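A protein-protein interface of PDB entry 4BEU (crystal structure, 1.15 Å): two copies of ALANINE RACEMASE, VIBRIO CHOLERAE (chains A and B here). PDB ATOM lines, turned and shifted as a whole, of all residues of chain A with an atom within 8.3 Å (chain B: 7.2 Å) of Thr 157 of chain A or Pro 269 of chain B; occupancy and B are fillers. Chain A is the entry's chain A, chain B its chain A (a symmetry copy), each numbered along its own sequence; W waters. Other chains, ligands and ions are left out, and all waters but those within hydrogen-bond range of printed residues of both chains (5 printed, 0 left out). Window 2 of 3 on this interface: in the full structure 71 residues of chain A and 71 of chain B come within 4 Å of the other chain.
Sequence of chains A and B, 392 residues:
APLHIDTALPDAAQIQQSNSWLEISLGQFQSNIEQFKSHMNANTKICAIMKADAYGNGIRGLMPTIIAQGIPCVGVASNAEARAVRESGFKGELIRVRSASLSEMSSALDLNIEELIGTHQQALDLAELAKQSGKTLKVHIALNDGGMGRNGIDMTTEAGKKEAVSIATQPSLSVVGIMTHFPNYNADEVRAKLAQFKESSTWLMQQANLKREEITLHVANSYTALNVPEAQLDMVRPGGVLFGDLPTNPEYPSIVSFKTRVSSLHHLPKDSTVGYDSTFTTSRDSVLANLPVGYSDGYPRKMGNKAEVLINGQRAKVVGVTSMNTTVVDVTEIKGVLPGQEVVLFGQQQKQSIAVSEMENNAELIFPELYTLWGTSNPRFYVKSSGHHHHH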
ATOM      1  N   ASN A 144     -36.649 -24.042 -23.763  1.00  0.00           N
ATOM      2  CA  ASN A 144     -36.520 -25.447 -23.410  1.00  0.00           C
ATOM      3  C   ASN A 144     -37.045 -25.861 -22.030  1.00  0.00           C
ATOM      4  O   ASN A 144     -36.661 -26.917 -21.548  1.00  0.00           O
ATOM      5  CB  ASN A 144     -35.062 -25.895 -23.562  1.00  0.00           C
ATOM      6  CG  ASN A 144     -34.923 -27.393 -23.678  1.00  0.00           C
ATOM      7  OD1 ASN A 144     -35.680 -28.052 -24.404  1.00  0.00           O
ATOM      8  ND2 ASN A 144     -33.922 -27.951 -22.996  1.00  0.00           N
ATOM      9  N   ILE A 153     -34.210 -22.877 -26.997  1.00  0.00           N
ATOM     10  CA  ILE A 153     -33.040 -22.414 -26.262  1.00  0.00           C
ATOM     11  C   ILE A 153     -33.169 -22.817 -24.800  1.00  0.00           C
ATOM     12  O   ILE A 153     -34.135 -22.483 -24.101  1.00  0.00           O
ATOM     13  CB  ILE A 153     -32.819 -20.887 -26.416  1.00  0.00           C
ATOM     14  CG1 ILE A 153     -31.568 -20.424 -25.659  1.00  0.00           C
ATOM     15  CG2 ILE A 153     -34.027 -20.074 -25.957  1.00  0.00           C
ATOM     16  CD1 ILE A 153     -30.298 -21.001 -26.188  1.00  0.00           C
ATOM     17  N   ASP A 154     -32.180 -23.560 -24.345  1.00  0.00           N
ATOM     18  CA  ASP A 154     -32.105 -23.913 -22.946  1.00  0.00           C
ATOM     19  C   ASP A 154     -31.566 -22.750 -22.141  1.00  0.00           C
ATOM     20  O   ASP A 154     -30.545 -22.156 -22.511  1.00  0.00           O
ATOM     21  CB  ASP A 154     -31.241 -25.143 -22.768  1.00  0.00           C
ATOM     22  CG  ASP A 154     -31.283 -25.650 -21.351  1.00  0.00           C
ATOM     23  OD1 ASP A 154     -30.465 -25.139 -20.530  1.00  0.00           O
ATOM     24  OD2 ASP A 154     -32.113 -26.527 -21.047  1.00  0.00           O
ATOM     25  N   MET A 155     -32.255 -22.429 -21.056  1.00  0.00           N
ATOM     26  CA  MET A 155     -31.900 -21.263 -20.252  1.00  0.00           C
ATOM     27  C   MET A 155     -31.476 -21.658 -18.834  1.00  0.00           C
ATOM     28  O   MET A 155     -31.496 -20.817 -17.923  1.00  0.00           O
ATOM     29  CB  MET A 155     -33.080 -20.306 -20.183  1.00  0.00           C
ATOM     30  CG  MET A 155     -33.400 -19.644 -21.518  1.00  0.00           C
ATOM     31  SD  MET A 155     -34.900 -18.689 -21.499  1.00  0.00           S
ATOM     32  CE  MET A 155     -34.603 -17.579 -20.153  1.00  0.00           C
ATOM     33  N   THR A 156     -31.059 -22.904 -18.638  1.00  0.00           N
ATOM     34  CA  THR A 156     -30.658 -23.364 -17.299  1.00  0.00           C
ATOM     35  C   THR A 156     -29.232 -22.973 -16.948  1.00  0.00           C
ATOM     36  O   THR A 156     -28.803 -23.185 -15.809  1.00  0.00           O
ATOM     37  CB  THR A 156     -30.812 -24.880 -17.122  1.00  0.00           C
ATOM     38  OG1 THR A 156     -29.876 -25.569 -17.953  1.00  0.00           O
ATOM     39  CG2 THR A 156     -32.248 -25.322 -17.428  1.00  0.00           C
ATOM     40  N   THR A 157     -28.508 -22.383 -17.889  1.00  0.00           N
ATOM     41  CA  THR A 157     -27.162 -21.886 -17.645  1.00  0.00           C
ATOM     42  C   THR A 157     -27.070 -20.439 -18.043  1.00  0.00           C
ATOM     43  O   THR A 157     -27.880 -19.916 -18.820  1.00  0.00           O
ATOM     44  CB  THR A 157     -26.111 -22.640 -18.484  1.00  0.00           C
ATOM     45  OG1 THR A 157     -26.314 -22.368 -19.885  1.00  0.00           O
ATOM     46  CG2 THR A 157     -26.171 -24.128 -18.230  1.00  0.00           C
ATOM     47  N   GLU A 158     -26.046 -19.783 -17.518  1.00  0.00           N
ATOM     48  CA  GLU A 158     -25.774 -18.403 -17.850  1.00  0.00           C
ATOM     49  C   GLU A 158     -25.621 -18.215 -19.374  1.00  0.00           C
ATOM     50  O   GLU A 158     -26.120 -17.248 -19.941  1.00  0.00           O
ATOM     51  CB  GLU A 158     -24.496 -17.980 -17.109  1.00  0.00           C
ATOM     52  CG  GLU A 158     -23.914 -16.641 -17.488  1.00  0.00           C
ATOM     53  CD  GLU A 158     -22.663 -16.326 -16.676  1.00  0.00           C
ATOM     54  OE1 GLU A 158     -22.279 -17.162 -15.826  1.00  0.00           O
ATOM     55  OE2 GLU A 158     -22.065 -15.251 -16.885  1.00  0.00           O
ATOM     56  N   ALA A 159     -24.908 -19.119 -20.021  1.00  0.00           N
ATOM     57  CA  ALA A 159     -24.715 -18.989 -21.464  1.00  0.00           C
ATOM     58  C   ALA A 159     -26.047 -19.081 -22.230  1.00  0.00           C
ATOM     59  O   ALA A 159     -26.264 -18.363 -23.204  1.00  0.00           O
ATOM     60  CB  ALA A 159     -23.744 -20.029 -21.967  1.00  0.00           C
ATOM     61  N   GLY A 160     -26.927 -19.964 -21.768  1.00  0.00           N
ATOM     62  CA  GLY A 160     -28.224 -20.150 -22.402  1.00  0.00           C
ATOM     63  C   GLY A 160     -29.101 -18.931 -22.223  1.00  0.00           C
ATOM     64  O   GLY A 160     -29.769 -18.479 -23.159  1.00  0.00           O
ATOM     65  N   LYS A 161     -29.102 -18.352 -21.019  1.00  0.00           N
ATOM     66  CA  LYS A 161     -29.857 -17.126 -20.772  1.00  0.00           C
ATOM     67  C   LYS A 161     -29.374 -15.978 -21.651  1.00  0.00           C
ATOM     68  O   LYS A 161     -30.171 -15.226 -22.208  1.00  0.00           O
ATOM     69  CB  LYS A 161     -29.768 -16.735 -19.295  1.00  0.00           C
ATOM     70  CG  LYS A 161     -30.639 -17.586 -18.431  1.00  0.00           C
ATOM     71  CD  LYS A 161     -30.625 -17.094 -16.994  1.00  0.00           C
ATOM     72  CE  LYS A 161     -31.415 -18.021 -16.112  1.00  0.00           C
ATOM     73  NZ  LYS A 161     -30.628 -19.251 -15.861  1.00  0.00           N
ATOM     74  N   LYS A 162     -28.058 -15.823 -21.742  1.00  0.00           N
ATOM     75  CA  LYS A 162     -27.465 -14.803 -22.584  1.00  0.00           C
ATOM     76  C   LYS A 162     -27.865 -14.999 -24.050  1.00  0.00           C
ATOM     77  O   LYS A 162     -28.199 -14.043 -24.733  1.00  0.00           O
ATOM     78  CB  LYS A 162     -25.949 -14.837 -22.426  1.00  0.00           C
ATOM     79  CG  LYS A 162     -25.232 -13.903 -23.371  1.00  0.00           C
ATOM     80  CD  LYS A 162     -23.733 -13.879 -23.127  1.00  0.00           C
ATOM     81  CE  LYS A 162     -23.060 -12.830 -24.008  1.00  0.00           C
ATOM     82  NZ  LYS A 162     -23.807 -11.534 -23.982  1.00  0.00           N
ATOM     83  N   GLU A 163     -27.835 -16.237 -24.533  1.00  0.00           N
ATOM     84  CA  GLU A 163     -28.264 -16.499 -25.904  1.00  0.00           C
ATOM     85  C   GLU A 163     -29.747 -16.193 -26.094  1.00  0.00           C
ATOM     86  O   GLU A 163     -30.121 -15.576 -27.094  1.00  0.00           O
ATOM     87  CB  GLU A 163     -27.905 -17.910 -26.331  1.00  0.00           C
ATOM     88  CG  GLU A 163     -28.296 -18.175 -27.765  1.00  0.00           C
ATOM     89  CD  GLU A 163     -27.771 -19.467 -28.321  1.00  0.00           C
ATOM     90  OE1 GLU A 163     -27.167 -20.261 -27.583  1.00  0.00           O
ATOM     91  OE2 GLU A 163     -27.982 -19.705 -29.535  1.00  0.00           O
ATOM     92  N   ALA A 164     -30.585 -16.557 -25.127  1.00  0.00           N
ATOM     93  CA  ALA A 164     -32.001 -16.241 -25.214  1.00  0.00           C
ATOM     94  C   ALA A 164     -32.248 -14.728 -25.327  1.00  0.00           C
ATOM     95  O   ALA A 164     -33.089 -14.271 -26.094  1.00  0.00           O
ATOM     96  CB  ALA A 164     -32.755 -16.812 -24.022  1.00  0.00           C
ATOM     97  N   TRP A 203     -38.805 -13.727 -17.075  1.00  0.00           N
ATOM     98  CA  TRP A 203     -37.451 -13.209 -17.000  1.00  0.00           C
ATOM     99  C   TRP A 203     -37.009 -12.690 -18.359  1.00  0.00           C
ATOM    100  O   TRP A 203     -36.477 -11.587 -18.476  1.00  0.00           O
ATOM    101  CB  TRP A 203     -36.506 -14.288 -16.530  1.00  0.00           C
ATOM    102  CG  TRP A 203     -35.099 -13.793 -16.379  1.00  0.00           C
ATOM    103  CD1 TRP A 203     -34.563 -13.167 -15.287  1.00  0.00           C
ATOM    104  CD2 TRP A 203     -34.051 -13.879 -17.352  1.00  0.00           C
ATOM    105  NE1 TRP A 203     -33.242 -12.868 -15.522  1.00  0.00           N
ATOM    106  CE2 TRP A 203     -32.903 -13.295 -16.780  1.00  0.00           C
ATOM    107  CE3 TRP A 203     -33.972 -14.392 -18.651  1.00  0.00           C
ATOM    108  CZ2 TRP A 203     -31.691 -13.202 -17.467  1.00  0.00           C
ATOM    109  CZ3 TRP A 203     -32.773 -14.304 -19.326  1.00  0.00           C
ATOM    110  CH2 TRP A 203     -31.646 -13.714 -18.739  1.00  0.00           C
ATOM    111  N   HIS B 266     -27.739 -26.382 -31.367  1.00  0.00           N
ATOM    112  CA  HIS B 266     -28.236 -26.018 -30.058  1.00  0.00           C
ATOM    113  C   HIS B 266     -27.296 -26.516 -28.971  1.00  0.00           C
ATOM    114  O   HIS B 266     -26.915 -27.674 -28.932  1.00  0.00           O
ATOM    115  CB  HIS B 266     -29.591 -26.685 -29.845  1.00  0.00           C
ATOM    116  CG  HIS B 266     -30.614 -26.314 -30.874  1.00  0.00           C
ATOM    117  ND1 HIS B 266     -31.689 -25.504 -30.596  1.00  0.00           N
ATOM    118  CD2 HIS B 266     -30.719 -26.635 -32.185  1.00  0.00           C
ATOM    119  CE1 HIS B 266     -32.405 -25.332 -31.693  1.00  0.00           C
ATOM    120  NE2 HIS B 266     -31.835 -26.005 -32.672  1.00  0.00           N
ATOM    121  N   HIS B 267     -26.965 -25.635 -28.036  1.00  0.00           N
ATOM    122  CA  HIS B 267     -26.150 -25.997 -26.865  1.00  0.00           C
ATOM    123  C   HIS B 267     -27.045 -26.468 -25.729  1.00  0.00           C
ATOM    124  O   HIS B 267     -27.943 -25.735 -25.299  1.00  0.00           O
ATOM    125  CB  HIS B 267     -25.303 -24.803 -26.417  1.00  0.00           C
ATOM    126  CG  HIS B 267     -24.226 -24.431 -27.390  1.00  0.00           C
ATOM    127  ND1 HIS B 267     -24.493 -23.910 -28.638  1.00  0.00           N
ATOM    128  CD2 HIS B 267     -22.878 -24.531 -27.304  1.00  0.00           C
ATOM    129  CE1 HIS B 267     -23.355 -23.694 -29.275  1.00  0.00           C
ATOM    130  NE2 HIS B 267     -22.360 -24.057 -28.486  1.00  0.00           N
ATOM    131  N   LEU B 268     -26.795 -27.676 -25.237  1.00  0.00           N
ATOM    132  CA  LEU B 268     -27.556 -28.264 -24.145  1.00  0.00           C
ATOM    133  C   LEU B 268     -26.600 -28.750 -23.076  1.00  0.00           C
ATOM    134  O   LEU B 268     -25.690 -29.538 -23.384  1.00  0.00           O
ATOM    135  CB  LEU B 268     -28.313 -29.491 -24.620  1.00  0.00           C
ATOM    136  CG  LEU B 268     -29.753 -29.392 -25.109  1.00  0.00           C
ATOM    137  CD1 LEU B 268     -30.333 -30.795 -25.105  1.00  0.00           C
ATOM    138  CD2 LEU B 268     -30.614 -28.479 -24.252  1.00  0.00           C
ATOM    139  N   PRO B 269     -26.807 -28.328 -21.821  1.00  0.00           N
ATOM    140  CA  PRO B 269     -25.896 -28.756 -20.752  1.00  0.00           C
ATOM    141  C   PRO B 269     -26.055 -30.225 -20.384  1.00  0.00           C
ATOM    142  O   PRO B 269     -27.021 -30.896 -20.773  1.00  0.00           O
ATOM    143  CB  PRO B 269     -26.297 -27.865 -19.566  1.00  0.00           C
ATOM    144  CG  PRO B 269     -27.719 -27.489 -19.827  1.00  0.00           C
ATOM    145  CD  PRO B 269     -27.895 -27.464 -21.327  1.00  0.00           C
ATOM    146  N   LYS B 270     -25.076 -30.734 -19.646  1.00  0.00           N
ATOM    147  CA  LYS B 270     -25.154 -32.050 -19.057  1.00  0.00           C
ATOM    148  C   LYS B 270     -26.488 -32.249 -18.345  1.00  0.00           C
ATOM    149  O   LYS B 270     -27.037 -31.300 -17.785  1.00  0.00           O
ATOM    150  CB  LYS B 270     -23.994 -32.206 -18.071  1.00  0.00           C
ATOM    151  CG  LYS B 270     -24.041 -33.452 -17.242  1.00  0.00           C
ATOM    152  CD  LYS B 270     -22.777 -33.569 -16.391  1.00  0.00           C
ATOM    153  CE  LYS B 270     -22.823 -34.814 -15.538  1.00  0.00           C
ATOM    154  NZ  LYS B 270     -21.468 -35.120 -15.022  1.00  0.00           N
ATOM    155  N   ASP B 271     -26.982 -33.487 -18.362  1.00  0.00           N
ATOM    156  CA  ASP B 271     -28.230 -33.880 -17.700  1.00  0.00           C
ATOM    157  C   ASP B 271     -29.499 -33.229 -18.305  1.00  0.00           C
ATOM    158  O   ASP B 271     -30.478 -32.961 -17.607  1.00  0.00           O
ATOM    159  CB  ASP B 271     -28.131 -33.622 -16.194  1.00  0.00           C
ATOM    160  CG  ASP B 271     -26.992 -34.400 -15.550  1.00  0.00           C
ATOM    161  OD1 ASP B 271     -26.798 -35.586 -15.909  1.00  0.00           O
ATOM    162  OD2 ASP B 271     -26.282 -33.826 -14.698  1.00  0.00           O
ATOM    163  N   SER B 272     -29.471 -32.991 -19.614  1.00  0.00           N
ATOM    164  CA  SER B 272     -30.631 -32.479 -20.354  1.00  0.00           C
ATOM    165  C   SER B 272     -31.301 -33.598 -21.146  1.00  0.00           C
ATOM    166  O   SER B 272     -30.632 -34.358 -21.838  1.00  0.00           O
ATOM    167  CB  SER B 272     -30.193 -31.397 -21.322  1.00  0.00           C
ATOM    168  OG  SER B 272     -29.655 -30.296 -20.617  1.00  0.00           O
ATOM    169  N   THR B 273     -32.616 -33.691 -21.048  1.00  0.00           N
ATOM    170  CA  THR B 273     -33.382 -34.684 -21.796  1.00  0.00           C
ATOM    171  C   THR B 273     -33.601 -34.266 -23.257  1.00  0.00           C
ATOM    172  O   THR B 273     -33.617 -33.078 -23.577  1.00  0.00           O
ATOM    173  CB  THR B 273     -34.742 -34.914 -21.142  1.00  0.00           C
ATOM    174  OG1 THR B 273     -35.366 -33.650 -20.899  1.00  0.00           O
ATOM    175  CG2 THR B 273     -34.569 -35.626 -19.802  1.00  0.00           C
ATOM    176  N   THR B 281     -30.645 -38.629 -22.260  1.00  0.00           N
ATOM    177  CA  THR B 281     -30.230 -37.542 -21.395  1.00  0.00           C
ATOM    178  C   THR B 281     -28.745 -37.315 -21.623  1.00  0.00           C
ATOM    179  O   THR B 281     -27.975 -38.269 -21.581  1.00  0.00           O
ATOM    180  CB  THR B 281     -30.472 -37.905 -19.917  1.00  0.00           C
ATOM    181  OG1 THR B 281     -31.868 -38.150 -19.717  1.00  0.00           O
ATOM    182  CG2 THR B 281     -30.016 -36.785 -18.984  1.00  0.00           C
ATOM    183  N   THR B 282     -28.333 -36.079 -21.880  1.00  0.00           N
ATOM    184  CA  THR B 282     -26.926 -35.776 -22.122  1.00  0.00           C
ATOM    185  C   THR B 282     -26.089 -36.097 -20.885  1.00  0.00           C
ATOM    186  O   THR B 282     -26.548 -35.911 -19.753  1.00  0.00           O
ATOM    187  CB  THR B 282     -26.710 -34.304 -22.454  1.00  0.00           C
ATOM    188  OG1 THR B 282     -27.218 -33.496 -21.380  1.00  0.00           O
ATOM    189  CG2 THR B 282     -27.395 -33.916 -23.781  1.00  0.00           C
ATOM    190  N   SER B 283     -24.876 -36.578 -21.111  1.00  0.00           N
ATOM    191  CA  SER B 283     -23.946 -36.910 -20.031  1.00  0.00           C
ATOM    192  C   SER B 283     -22.838 -35.864 -19.924  1.00  0.00           C
ATOM    193  O   SER B 283     -21.907 -36.011 -19.128  1.00  0.00           O
ATOM    194  CB  SER B 283     -23.310 -38.266 -20.308  1.00  0.00           C
ATOM    195  OG  SER B 283     -22.529 -38.196 -21.488  1.00  0.00           O
ATOM    196  N   ARG B 284     -22.942 -34.808 -20.726  1.00  0.00           N
ATOM    197  CA  ARG B 284     -21.902 -33.808 -20.861  1.00  0.00           C
ATOM    198  C   ARG B 284     -22.533 -32.595 -21.523  1.00  0.00           C
ATOM    199  O   ARG B 284     -23.597 -32.710 -22.150  1.00  0.00           O
ATOM    200  CB  ARG B 284     -20.773 -34.338 -21.750  1.00  0.00           C
ATOM    201  CG  ARG B 284     -21.250 -34.671 -23.162  1.00  0.00           C
ATOM    202  CD  ARG B 284     -20.160 -35.241 -24.047  1.00  0.00           C
ATOM    203  NE  ARG B 284     -20.723 -35.650 -25.336  1.00  0.00           N
ATOM    204  CZ  ARG B 284     -20.052 -36.293 -26.285  1.00  0.00           C
ATOM    205  NH1 ARG B 284     -18.774 -36.606 -26.107  1.00  0.00           N
ATOM    206  NH2 ARG B 284     -20.657 -36.625 -27.421  1.00  0.00           N
ATOM    207  N   ASP B 285     -21.912 -31.437 -21.406  1.00  0.00           N
ATOM    208  CA  ASP B 285     -22.361 -30.293 -22.170  1.00  0.00           C
ATOM    209  C   ASP B 285     -22.231 -30.664 -23.646  1.00  0.00           C
ATOM    210  O   ASP B 285     -21.187 -31.159 -24.091  1.00  0.00           O
ATOM    211  CB  ASP B 285     -21.545 -29.042 -21.841  1.00  0.00           C
ATOM    212  CG  ASP B 285     -21.823 -28.498 -20.440  1.00  0.00           C
ATOM    213  OD1 ASP B 285     -22.742 -28.984 -19.753  1.00  0.00           O
ATOM    214  OD2 ASP B 285     -21.107 -27.561 -20.034  1.00  0.00           O
ATOM    215  N   SER B 286     -23.296 -30.424 -24.403  1.00  0.00           N
ATOM    216  CA  SER B 286     -23.427 -30.959 -25.751  1.00  0.00           C
ATOM    217  C   SER B 286     -23.756 -29.875 -26.768  1.00  0.00           C
ATOM    218  O   SER B 286     -24.284 -28.814 -26.428  1.00  0.00           O
ATOM    219  CB  SER B 286     -24.543 -32.004 -25.766  1.00  0.00           C
ATOM    220  OG  SER B 286     -24.285 -33.056 -24.834  1.00  0.00           O
HETATM  221  O   HOH W   1     -33.718 -30.651 -22.406  1.00  0.00           O
HETATM  222  O   HOH W   2     -28.080 -23.183 -23.931  1.00  0.00           O
HETATM  223  O   HOH W   3     -30.509 -25.086 -26.253  1.00  0.00           O
HETATM  224  O   HOH W   4     -31.410 -28.616 -19.414  1.00  0.00           O
HETATM  225  O   HOH W   5     -27.702 -22.883 -28.280  1.00  0.00           O
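Among the printed residues, pairs that only touch across the chains: Asn 144 of chain A with Leu 268 of chain B (3.6 Å), Asp 154 of chain A with Leu 268 of chain B (3.7 Å), Asp 154 of chain A with Pro 269 of chain B (3.6 Å), Thr 156 of chain A with Pro 269 of chain B (3.4 Å) and Thr 157 of chain A with Pro 269 of chain B (3.97 Å).
O of Ile 153 of chain A lies within hydrogen-bond range of N of Asn 144 of chain A. The side-chain carboxylate (OD1) of Asp 154 of chain A is in hydrogen-bond range of the side-chain hydroxyl (OG1) of Thr 156 of chain A, 2.7 Å away. The side-chain carboxylate of Asp 154 of chain A is in hydrogen-bond range of the side-chain amide nitrogen of Asn 144 of chain A (3.0 Å). The backbone carbonyl oxygen (O) of Leu 268 of chain B sits at hydrogen-bond distance from the backbone NH (N) of Ser 286 of chain B, at 2.7 Å. OG1 of Thr 157 of chain A lies within hydrogen-bond range of N of Gly 160 of chain A, at 3.1 Å. The backbone carbonyl oxygen of Pro 269 of chain B is in hydrogen-bond range of the side-chain hydroxyl of Ser 272 of chain B.
No position is printed for both chains.
Water W1 bridges O of Thr 273 of chain B (2.7 Å) and ND2 of Asn 144 of chain A (2.8 Å). Water W4 lies within hydrogen-bond range of OG of Ser 272 of chain B (2.7 Å) and OD2 of Asp 154 of chain A (2.7 Å). Water W5 lies within hydrogen-bond range of OE1 of Glu 163 of chain A and N of His 267 of chain B. Water W3 bridges the backbone carbonyl oxygen of His 267 of chain B (2.8 Å) and the backbone NH of Asp 154 of chain A (3.0 Å). Water W2 bridges the backbone carbonyl oxygen of His 267 of chain B (2.9 Å) and the backbone carbonyl oxygen of Asp 154 of chain A (3.0 Å).
Of chain A, only Asp 154, Thr 156 and Thr 157 come within 4 Å of Pro 269 of chain B. Of the printed residues of chain B, Asp 154 of chain A touches Leu 268 and Pro 269. Of the printed residues of chain B, Asn 144 of chain A touches Leu 268. Printed residues of chain B within 4 Å of Thr 156 of chain A: Pro 269 (3.4 Å). Of the printed residues of chain A, Leu 268 of chain B touches Asn 144 (3.6 Å) and Asp 154 (3.7 Å). Thr 281 of chain B touches none of the printed residues of chain A. The nearest residue of chain B that does not touch Thr 157 of chain A is Asp 285 of chain B (6.1 Å).
Of the 14 printed residues of chain B, 2 touch a printed residue of chain A. Hydrophobic or aromatic side chains of chain B within 4 Å of the printed part of chain A: Leu 268 and Pro 269. Among the printed residues, 5 pairs touch across the chains. Among the printed residues, no Asp or Glu carboxylate lies within 4 Å of a Lys or Arg side-chain nitrogen of the other chain.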
